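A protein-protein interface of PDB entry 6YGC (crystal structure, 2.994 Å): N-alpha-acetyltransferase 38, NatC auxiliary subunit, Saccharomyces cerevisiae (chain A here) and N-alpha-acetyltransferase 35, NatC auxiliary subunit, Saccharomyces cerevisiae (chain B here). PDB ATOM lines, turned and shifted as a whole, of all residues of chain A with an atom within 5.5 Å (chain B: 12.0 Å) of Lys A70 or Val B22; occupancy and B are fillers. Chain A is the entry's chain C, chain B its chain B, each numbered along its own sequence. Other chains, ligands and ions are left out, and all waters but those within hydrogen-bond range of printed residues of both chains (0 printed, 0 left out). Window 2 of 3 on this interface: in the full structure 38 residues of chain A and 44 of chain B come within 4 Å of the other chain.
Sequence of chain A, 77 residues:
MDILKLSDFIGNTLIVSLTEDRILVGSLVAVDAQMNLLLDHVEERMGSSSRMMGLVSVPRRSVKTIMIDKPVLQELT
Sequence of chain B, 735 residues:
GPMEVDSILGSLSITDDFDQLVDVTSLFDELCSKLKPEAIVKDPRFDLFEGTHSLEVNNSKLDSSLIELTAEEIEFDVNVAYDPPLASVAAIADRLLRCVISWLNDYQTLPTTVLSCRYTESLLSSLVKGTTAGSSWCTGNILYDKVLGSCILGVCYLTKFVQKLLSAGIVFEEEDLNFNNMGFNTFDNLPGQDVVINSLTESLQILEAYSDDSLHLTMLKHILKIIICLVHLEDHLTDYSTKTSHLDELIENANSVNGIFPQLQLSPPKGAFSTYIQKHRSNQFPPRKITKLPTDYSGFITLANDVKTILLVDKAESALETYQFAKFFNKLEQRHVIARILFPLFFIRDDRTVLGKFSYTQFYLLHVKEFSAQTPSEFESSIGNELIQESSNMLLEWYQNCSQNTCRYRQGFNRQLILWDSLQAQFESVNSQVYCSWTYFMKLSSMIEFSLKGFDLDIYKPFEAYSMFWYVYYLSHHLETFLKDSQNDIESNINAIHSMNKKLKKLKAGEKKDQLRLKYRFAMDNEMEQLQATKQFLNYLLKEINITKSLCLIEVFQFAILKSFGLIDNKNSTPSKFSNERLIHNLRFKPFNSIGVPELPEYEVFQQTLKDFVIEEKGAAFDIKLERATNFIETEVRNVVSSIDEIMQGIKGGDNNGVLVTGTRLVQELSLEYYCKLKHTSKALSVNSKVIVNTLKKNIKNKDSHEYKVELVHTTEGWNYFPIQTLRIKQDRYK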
ATOM      1  N   ILE A  66      17.319   4.390  26.414  1.00  0.00           N
ATOM      2  CA  ILE A  66      18.013   5.650  26.651  1.00  0.00           C
ATOM      3  C   ILE A  66      19.440   5.334  27.072  1.00  0.00           C
ATOM      4  O   ILE A  66      19.655   4.545  27.998  1.00  0.00           O
ATOM      5  CB  ILE A  66      17.312   6.500  27.728  1.00  0.00           C
ATOM      6  CG1 ILE A  66      15.847   6.734  27.361  1.00  0.00           C
ATOM      7  CG2 ILE A  66      18.036   7.829  27.910  1.00  0.00           C
ATOM      8  CD1 ILE A  66      15.071   7.485  28.421  1.00  0.00           C
ATOM      9  N   MET A  67      20.411   5.951  26.400  1.00  0.00           N
ATOM     10  CA  MET A  67      21.817   5.704  26.683  1.00  0.00           C
ATOM     11  C   MET A  67      22.573   7.022  26.757  1.00  0.00           C
ATOM     12  O   MET A  67      22.246   7.982  26.058  1.00  0.00           O
ATOM     13  CB  MET A  67      22.451   4.791  25.625  1.00  0.00           C
ATOM     14  CG  MET A  67      21.849   3.395  25.574  1.00  0.00           C
ATOM     15  SD  MET A  67      22.660   2.330  24.368  1.00  0.00           S
ATOM     16  CE  MET A  67      21.723   0.817  24.571  1.00  0.00           C
ATOM     17  N   ILE A  68      23.597   7.054  27.611  1.00  0.00           N
ATOM     18  CA  ILE A  68      24.430   8.235  27.801  1.00  0.00           C
ATOM     19  C   ILE A  68      25.890   7.842  27.626  1.00  0.00           C
ATOM     20  O   ILE A  68      26.297   6.721  27.946  1.00  0.00           O
ATOM     21  CB  ILE A  68      24.193   8.891  29.185  1.00  0.00           C
ATOM     22  CG1 ILE A  68      24.915  10.237  29.284  1.00  0.00           C
ATOM     23  CG2 ILE A  68      24.639   7.964  30.313  1.00  0.00           C
ATOM     24  CD1 ILE A  68      24.794  10.906  30.636  1.00  0.00           C
ATOM     25  N   ASP A  69      26.678   8.772  27.091  1.00  0.00           N
ATOM     26  CA  ASP A  69      28.111   8.554  26.932  1.00  0.00           C
ATOM     27  C   ASP A  69      28.763   8.375  28.300  1.00  0.00           C
ATOM     28  O   ASP A  69      28.464   9.106  29.248  1.00  0.00           O
ATOM     29  CB  ASP A  69      28.735   9.732  26.183  1.00  0.00           C
ATOM     30  CG  ASP A  69      30.060   9.383  25.533  1.00  0.00           C
ATOM     31  OD1 ASP A  69      30.516   8.234  25.684  1.00  0.00           O
ATOM     32  OD2 ASP A  69      30.645  10.260  24.863  1.00  0.00           O
ATOM     33  N   LYS A  70      29.652   7.384  28.405  1.00  0.00           N
ATOM     34  CA  LYS A  70      30.248   7.025  29.687  1.00  0.00           C
ATOM     35  C   LYS A  70      31.163   8.126  30.229  1.00  0.00           C
ATOM     36  O   LYS A  70      31.092   8.439  31.422  1.00  0.00           O
ATOM     37  CB  LYS A  70      31.010   5.702  29.584  1.00  0.00           C
ATOM     38  CG  LYS A  70      31.057   4.910  30.886  1.00  0.00           C
ATOM     39  CD  LYS A  70      32.033   3.746  30.809  1.00  0.00           C
ATOM     40  CE  LYS A  70      31.686   2.664  31.820  1.00  0.00           C
ATOM     41  NZ  LYS A  70      30.465   1.904  31.429  1.00  0.00           N
ATOM     42  N   PRO A  71      32.036   8.732  29.409  1.00  0.00           N
ATOM     43  CA  PRO A  71      32.816   9.875  29.920  1.00  0.00           C
ATOM     44  C   PRO A  71      31.952  11.015  30.429  1.00  0.00           C
ATOM     45  O   PRO A  71      32.303  11.660  31.425  1.00  0.00           O
ATOM     46  CB  PRO A  71      33.655  10.293  28.705  1.00  0.00           C
ATOM     47  CG  PRO A  71      33.817   9.034  27.934  1.00  0.00           C
ATOM     48  CD  PRO A  71      32.506   8.321  28.070  1.00  0.00           C
ATOM     49  N   VAL A  72      30.818  11.276  29.776  1.00  0.00           N
ATOM     50  CA  VAL A  72      29.938  12.351  30.223  1.00  0.00           C
ATOM     51  C   VAL A  72      29.309  12.001  31.565  1.00  0.00           C
ATOM     52  O   VAL A  72      29.131  12.870  32.427  1.00  0.00           O
ATOM     53  CB  VAL A  72      28.872  12.648  29.153  1.00  0.00           C
ATOM     54  CG1 VAL A  72      27.923  13.739  29.631  1.00  0.00           C
ATOM     55  CG2 VAL A  72      29.531  13.051  27.844  1.00  0.00           C
ATOM     56  N   LEU A  73      28.987  10.722  31.772  1.00  0.00           N
ATOM     57  CA  LEU A  73      28.280  10.314  32.983  1.00  0.00           C
ATOM     58  C   LEU A  73      29.127  10.528  34.232  1.00  0.00           C
ATOM     59  O   LEU A  73      28.599  10.886  35.292  1.00  0.00           O
ATOM     60  CB  LEU A  73      27.858   8.849  32.869  1.00  0.00           C
ATOM     61  CG  LEU A  73      27.181   8.233  34.095  1.00  0.00           C
ATOM     62  CD1 LEU A  73      25.921   9.005  34.454  1.00  0.00           C
ATOM     63  CD2 LEU A  73      26.867   6.764  33.857  1.00  0.00           C
ATOM     64  N   GLN A  74      30.441  10.322  34.131  1.00  0.00           N
ATOM     65  CA  GLN A  74      31.287  10.391  35.317  1.00  0.00           C
ATOM     66  C   GLN A  74      31.536  11.825  35.772  1.00  0.00           C
ATOM     67  O   GLN A  74      31.723  12.063  36.970  1.00  0.00           O
ATOM     68  CB  GLN A  74      32.616   9.680  35.058  1.00  0.00           C
ATOM     69  CG  GLN A  74      32.485   8.342  34.332  1.00  0.00           C
ATOM     70  CD  GLN A  74      31.611   7.333  35.063  1.00  0.00           C
ATOM     71  OE1 GLN A  74      31.385   7.442  36.270  1.00  0.00           O
ATOM     72  NE2 GLN A  74      31.118   6.342  34.331  1.00  0.00           N
ATOM     73  N   THR B  15      26.563   4.970  15.923  1.00  0.00           N
ATOM     74  CA  THR B  15      27.095   4.966  17.278  1.00  0.00           C
ATOM     75  C   THR B  15      28.604   5.184  17.312  1.00  0.00           C
ATOM     76  O   THR B  15      29.170   5.347  18.399  1.00  0.00           O
ATOM     77  CB  THR B  15      26.741   3.640  17.974  1.00  0.00           C
ATOM     78  OG1 THR B  15      25.384   3.285  17.673  1.00  0.00           O
ATOM     79  CG2 THR B  15      26.888   3.749  19.488  1.00  0.00           C
ATOM     80  N   ASP B  16      29.260   5.222  16.148  1.00  0.00           N
ATOM     81  CA  ASP B  16      30.718   5.267  16.102  1.00  0.00           C
ATOM     82  C   ASP B  16      31.288   6.521  16.755  1.00  0.00           C
ATOM     83  O   ASP B  16      32.395   6.479  17.304  1.00  0.00           O
ATOM     84  CB  ASP B  16      31.200   5.168  14.656  1.00  0.00           C
ATOM     85  CG  ASP B  16      31.396   3.735  14.204  1.00  0.00           C
ATOM     86  OD1 ASP B  16      31.100   2.815  14.997  1.00  0.00           O
ATOM     87  OD2 ASP B  16      31.856   3.529  13.061  1.00  0.00           O
ATOM     88  N   ASP B  17      30.566   7.643  16.702  1.00  0.00           N
ATOM     89  CA  ASP B  17      31.109   8.885  17.245  1.00  0.00           C
ATOM     90  C   ASP B  17      31.296   8.798  18.756  1.00  0.00           C
ATOM     91  O   ASP B  17      32.273   9.328  19.299  1.00  0.00           O
ATOM     92  CB  ASP B  17      30.206  10.061  16.874  1.00  0.00           C
ATOM     93  CG  ASP B  17      28.735   9.739  17.031  1.00  0.00           C
ATOM     94  OD1 ASP B  17      28.402   8.542  17.161  1.00  0.00           O
ATOM     95  OD2 ASP B  17      27.915  10.679  17.026  1.00  0.00           O
ATOM     96  N   PHE B  18      30.379   8.132  19.452  1.00  0.00           N
ATOM     97  CA  PHE B  18      30.479   7.961  20.895  1.00  0.00           C
ATOM     98  C   PHE B  18      31.255   6.687  21.211  1.00  0.00           C
ATOM     99  O   PHE B  18      30.926   5.610  20.703  1.00  0.00           O
ATOM    100  CB  PHE B  18      29.089   7.917  21.530  1.00  0.00           C
ATOM    101  CG  PHE B  18      28.271   9.149  21.270  1.00  0.00           C
ATOM    102  CD1 PHE B  18      28.428  10.279  22.056  1.00  0.00           C
ATOM    103  CD2 PHE B  18      27.349   9.179  20.238  1.00  0.00           C
ATOM    104  CE1 PHE B  18      27.678  11.415  21.817  1.00  0.00           C
ATOM    105  CE2 PHE B  18      26.599  10.309  19.995  1.00  0.00           C
ATOM    106  CZ  PHE B  18      26.762  11.430  20.785  1.00  0.00           C
ATOM    107  N   ASP B  19      32.282   6.816  22.055  1.00  0.00           N
ATOM    108  CA  ASP B  19      33.177   5.691  22.312  1.00  0.00           C
ATOM    109  C   ASP B  19      32.521   4.634  23.195  1.00  0.00           C
ATOM    110  O   ASP B  19      32.678   3.432  22.950  1.00  0.00           O
ATOM    111  CB  ASP B  19      34.475   6.188  22.948  1.00  0.00           C
ATOM    112  CG  ASP B  19      35.270   7.093  22.025  1.00  0.00           C
ATOM    113  OD1 ASP B  19      34.746   7.457  20.951  1.00  0.00           O
ATOM    114  OD2 ASP B  19      36.419   7.436  22.372  1.00  0.00           O
ATOM    115  N   GLN B  20      31.792   5.053  24.228  1.00  0.00           N
ATOM    116  CA  GLN B  20      31.183   4.119  25.165  1.00  0.00           C
ATOM    117  C   GLN B  20      29.764   4.561  25.488  1.00  0.00           C
ATOM    118  O   GLN B  20      29.510   5.749  25.697  1.00  0.00           O
ATOM    119  CB  GLN B  20      32.006   4.008  26.455  1.00  0.00           C
ATOM    120  CG  GLN B  20      33.377   3.371  26.266  1.00  0.00           C
ATOM    121  CD  GLN B  20      34.212   3.386  27.532  1.00  0.00           C
ATOM    122  OE1 GLN B  20      34.138   4.322  28.327  1.00  0.00           O
ATOM    123  NE2 GLN B  20      35.011   2.343  27.726  1.00  0.00           N
ATOM    124  N   LEU B  21      28.841   3.601  25.535  1.00  0.00           N
ATOM    125  CA  LEU B  21      27.446   3.886  25.836  1.00  0.00           C
ATOM    126  C   LEU B  21      26.967   3.016  26.987  1.00  0.00           C
ATOM    127  O   LEU B  21      27.294   1.828  27.062  1.00  0.00           O
ATOM    128  CB  LEU B  21      26.549   3.665  24.612  1.00  0.00           C
ATOM    129  CG  LEU B  21      26.571   4.753  23.536  1.00  0.00           C
ATOM    130  CD1 LEU B  21      25.384   4.587  22.602  1.00  0.00           C
ATOM    131  CD2 LEU B  21      26.575   6.141  24.161  1.00  0.00           C
ATOM    132  N   VAL B  22      26.184   3.616  27.882  1.00  0.00           N
ATOM    133  CA  VAL B  22      25.613   2.930  29.034  1.00  0.00           C
ATOM    134  C   VAL B  22      24.099   3.056  28.960  1.00  0.00           C
ATOM    135  O   VAL B  22      23.573   4.163  28.808  1.00  0.00           O
ATOM    136  CB  VAL B  22      26.137   3.510  30.360  1.00  0.00           C
ATOM    137  CG1 VAL B  22      25.693   2.645  31.528  1.00  0.00           C
ATOM    138  CG2 VAL B  22      27.651   3.645  30.325  1.00  0.00           C
ATOM    139  N   ASP B  23      23.403   1.927  29.072  1.00  0.00           N
ATOM    140  CA  ASP B  23      21.946   1.944  29.063  1.00  0.00           C
ATOM    141  C   ASP B  23      21.424   2.493  30.386  1.00  0.00           C
ATOM    142  O   ASP B  23      21.790   2.007  31.460  1.00  0.00           O
ATOM    143  CB  ASP B  23      21.400   0.539  28.812  1.00  0.00           C
ATOM    144  CG  ASP B  23      19.892   0.521  28.621  1.00  0.00           C
ATOM    145  OD1 ASP B  23      19.266   1.600  28.661  1.00  0.00           O
ATOM    146  OD2 ASP B  23      19.333  -0.578  28.427  1.00  0.00           O
ATOM    147  N   VAL B  24      20.566   3.510  30.305  1.00  0.00           N
ATOM    148  CA  VAL B  24      20.006   4.167  31.477  1.00  0.00           C
ATOM    149  C   VAL B  24      18.488   4.050  31.526  1.00  0.00           C
ATOM    150  O   VAL B  24      17.846   4.712  32.340  1.00  0.00           O
ATOM    151  CB  VAL B  24      20.438   5.647  31.544  1.00  0.00           C
ATOM    152  CG1 VAL B  24      20.603   6.090  32.989  1.00  0.00           C
ATOM    153  CG2 VAL B  24      21.723   5.869  30.767  1.00  0.00           C
ATOM    154  N   THR B  25      17.899   3.211  30.670  1.00  0.00           N
ATOM    155  CA  THR B  25      16.444   3.123  30.603  1.00  0.00           C
ATOM    156  C   THR B  25      15.859   2.580  31.902  1.00  0.00           C
ATOM    157  O   THR B  25      14.832   3.074  32.383  1.00  0.00           O
ATOM    158  CB  THR B  25      16.030   2.247  29.421  1.00  0.00           C
ATOM    159  OG1 THR B  25      16.745   2.666  28.254  1.00  0.00           O
ATOM    160  CG2 THR B  25      14.533   2.372  29.164  1.00  0.00           C
ATOM    161  N   SER B  26      16.498   1.562  32.483  1.00  0.00           N
ATOM    162  CA  SER B  26      16.034   1.029  33.759  1.00  0.00           C
ATOM    163  C   SER B  26      16.165   2.057  34.875  1.00  0.00           C
ATOM    164  O   SER B  26      15.335   2.088  35.791  1.00  0.00           O
ATOM    165  CB  SER B  26      16.808  -0.243  34.105  1.00  0.00           C
ATOM    166  OG  SER B  26      18.206  -0.021  34.039  1.00  0.00           O
ATOM    167  N   LEU B  27      17.188   2.913  34.808  1.00  0.00           N
ATOM    168  CA  LEU B  27      17.354   3.949  35.821  1.00  0.00           C
ATOM    169  C   LEU B  27      16.283   5.023  35.687  1.00  0.00           C
ATOM    170  O   LEU B  27      15.718   5.476  36.689  1.00  0.00           O
ATOM    171  CB  LEU B  27      18.753   4.560  35.710  1.00  0.00           C
ATOM    172  CG  LEU B  27      19.465   5.091  36.960  1.00  0.00           C
ATOM    173  CD1 LEU B  27      20.901   5.463  36.627  1.00  0.00           C
ATOM    174  CD2 LEU B  27      18.746   6.279  37.566  1.00  0.00           C
ATOM    175  N   PHE B  28      15.985   5.436  34.452  1.00  0.00           N
ATOM    176  CA  PHE B  28      15.010   6.501  34.234  1.00  0.00           C
ATOM    177  C   PHE B  28      13.611   6.076  34.662  1.00  0.00           C
ATOM    178  O   PHE B  28      12.873   6.870  35.258  1.00  0.00           O
ATOM    179  CB  PHE B  28      15.012   6.920  32.764  1.00  0.00           C
ATOM    180  CG  PHE B  28      15.966   8.037  32.451  1.00  0.00           C
ATOM    181  CD1 PHE B  28      17.331   7.871  32.617  1.00  0.00           C
ATOM    182  CD2 PHE B  28      15.496   9.250  31.975  1.00  0.00           C
ATOM    183  CE1 PHE B  28      18.209   8.900  32.325  1.00  0.00           C
ATOM    184  CE2 PHE B  28      16.368  10.280  31.681  1.00  0.00           C
ATOM    185  CZ  PHE B  28      17.726  10.106  31.855  1.00  0.00           C
ATOM    186  N   ASP B  29      13.229   4.830  34.368  1.00  0.00           N
ATOM    187  CA  ASP B  29      11.876   4.375  34.674  1.00  0.00           C
ATOM    188  C   ASP B  29      11.604   4.421  36.172  1.00  0.00           C
ATOM    189  O   ASP B  29      10.562   4.923  36.610  1.00  0.00           O
ATOM    190  CB  ASP B  29      11.664   2.962  34.131  1.00  0.00           C
ATOM    191  CG  ASP B  29      10.234   2.476  34.308  1.00  0.00           C
ATOM    192  OD1 ASP B  29       9.340   3.315  34.545  1.00  0.00           O
ATOM    193  OD2 ASP B  29      10.006   1.252  34.214  1.00  0.00           O
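The backbone carbonyl oxygen of Gln B20 lies close to the side-chain carboxylate of Asp A69, 2.7 Å away. The backbone NH of Lys A70 sits at hydrogen-bond distance from the backbone carbonyl oxygen of Gln B20, 3.2 Å away. N of Val B22 is in hydrogen-bond range of O of Ile A68. N of Val B24 sits at hydrogen-bond distance from O of Ile A66, at 2.7 Å. OG1 of Thr B25 is in hydrogen-bond range of N of Ile A66, at 2.6 Å. The side-chain carboxylate (OD1) of Asp B23 sits close to the backbone carbonyl oxygen (O) of Ile A66 (3.0 Å).
The side-chain hydroxyl (OG1) of Thr B25 is in hydrogen-bond range of the side-chain carboxylate (OD1) of Asp B23 (2.8 Å).
Among the printed residues, pairs that only touch across the chains: Met A67 with Val B22 (3.2 Å), Lys A70 with Val B22 (3.5 Å), Asp A69 with Phe B18 (3.6 Å), Ile A68 with Val B24 (3.6 Å), Ile A68 with Leu B21 (3.7 Å), Met A67 with Asp B23 (3.8 Å), Asp A69 with Leu B21 (3.9 Å), Met A67 with Leu B21 (3.95 Å) and Ile A66 with Phe B28 (3.99 Å).
Printed residues of chain A within 4 Å of Val B22: Met A67 (3.2 Å), Ile A68 (3.1 Å) and Lys A70 (3.5 Å). Of chain B, only Leu B21, Val B22 and Asp B23 come within 4 Å of Met A67. Ile A68 touches three residues of chain B. Printed residues of chain B within 4 Å of Asp A69: Phe B18 (3.6 Å), Gln B20 (2.7 Å) and Leu B21 (3.9 Å). No residue of chain B comes within 4 Å of Pro A71. No residue of chain B comes within 4 Å of Val A72. No residue of chain B comes within 4 Å of Leu A73. Of the printed residues of chain A, Leu B21 touches Met A67 (3.95 Å), Ile A68 (3.7 Å) and Asp A69 (3.9 Å). Printed residues of chain A within 4 Å of Phe B28: Ile A66. Of the printed residues of chain B, Ile A66 touches Asp B23 (3.0 Å), Val B24 (2.7 Å), Thr B25 (2.6 Å) and Phe B28 (3.99 Å). Thr B15 touches none of the printed residues of chain A. Ser B26 touches none of the printed residues of chain A.
Of the 9 printed residues of chain A, 5 touch a printed residue of chain B. Hydrophobic or aromatic side chains of chain A within 4 Å of the printed part of chain B: Ile A66, Met A67 and Ile A68. Of the 15 printed residues of chain B, 8 touch a printed residue of chain A. Hydrophobic or aromatic side chains of chain B that line the printed part of chain A: Phe B18, Leu B21, Val B22, Val B24 and Phe B28. Among the printed residues, no Asp or Glu carboxylate lies within 4 Å of a Lys or Arg side-chain nitrogen of the other chain.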
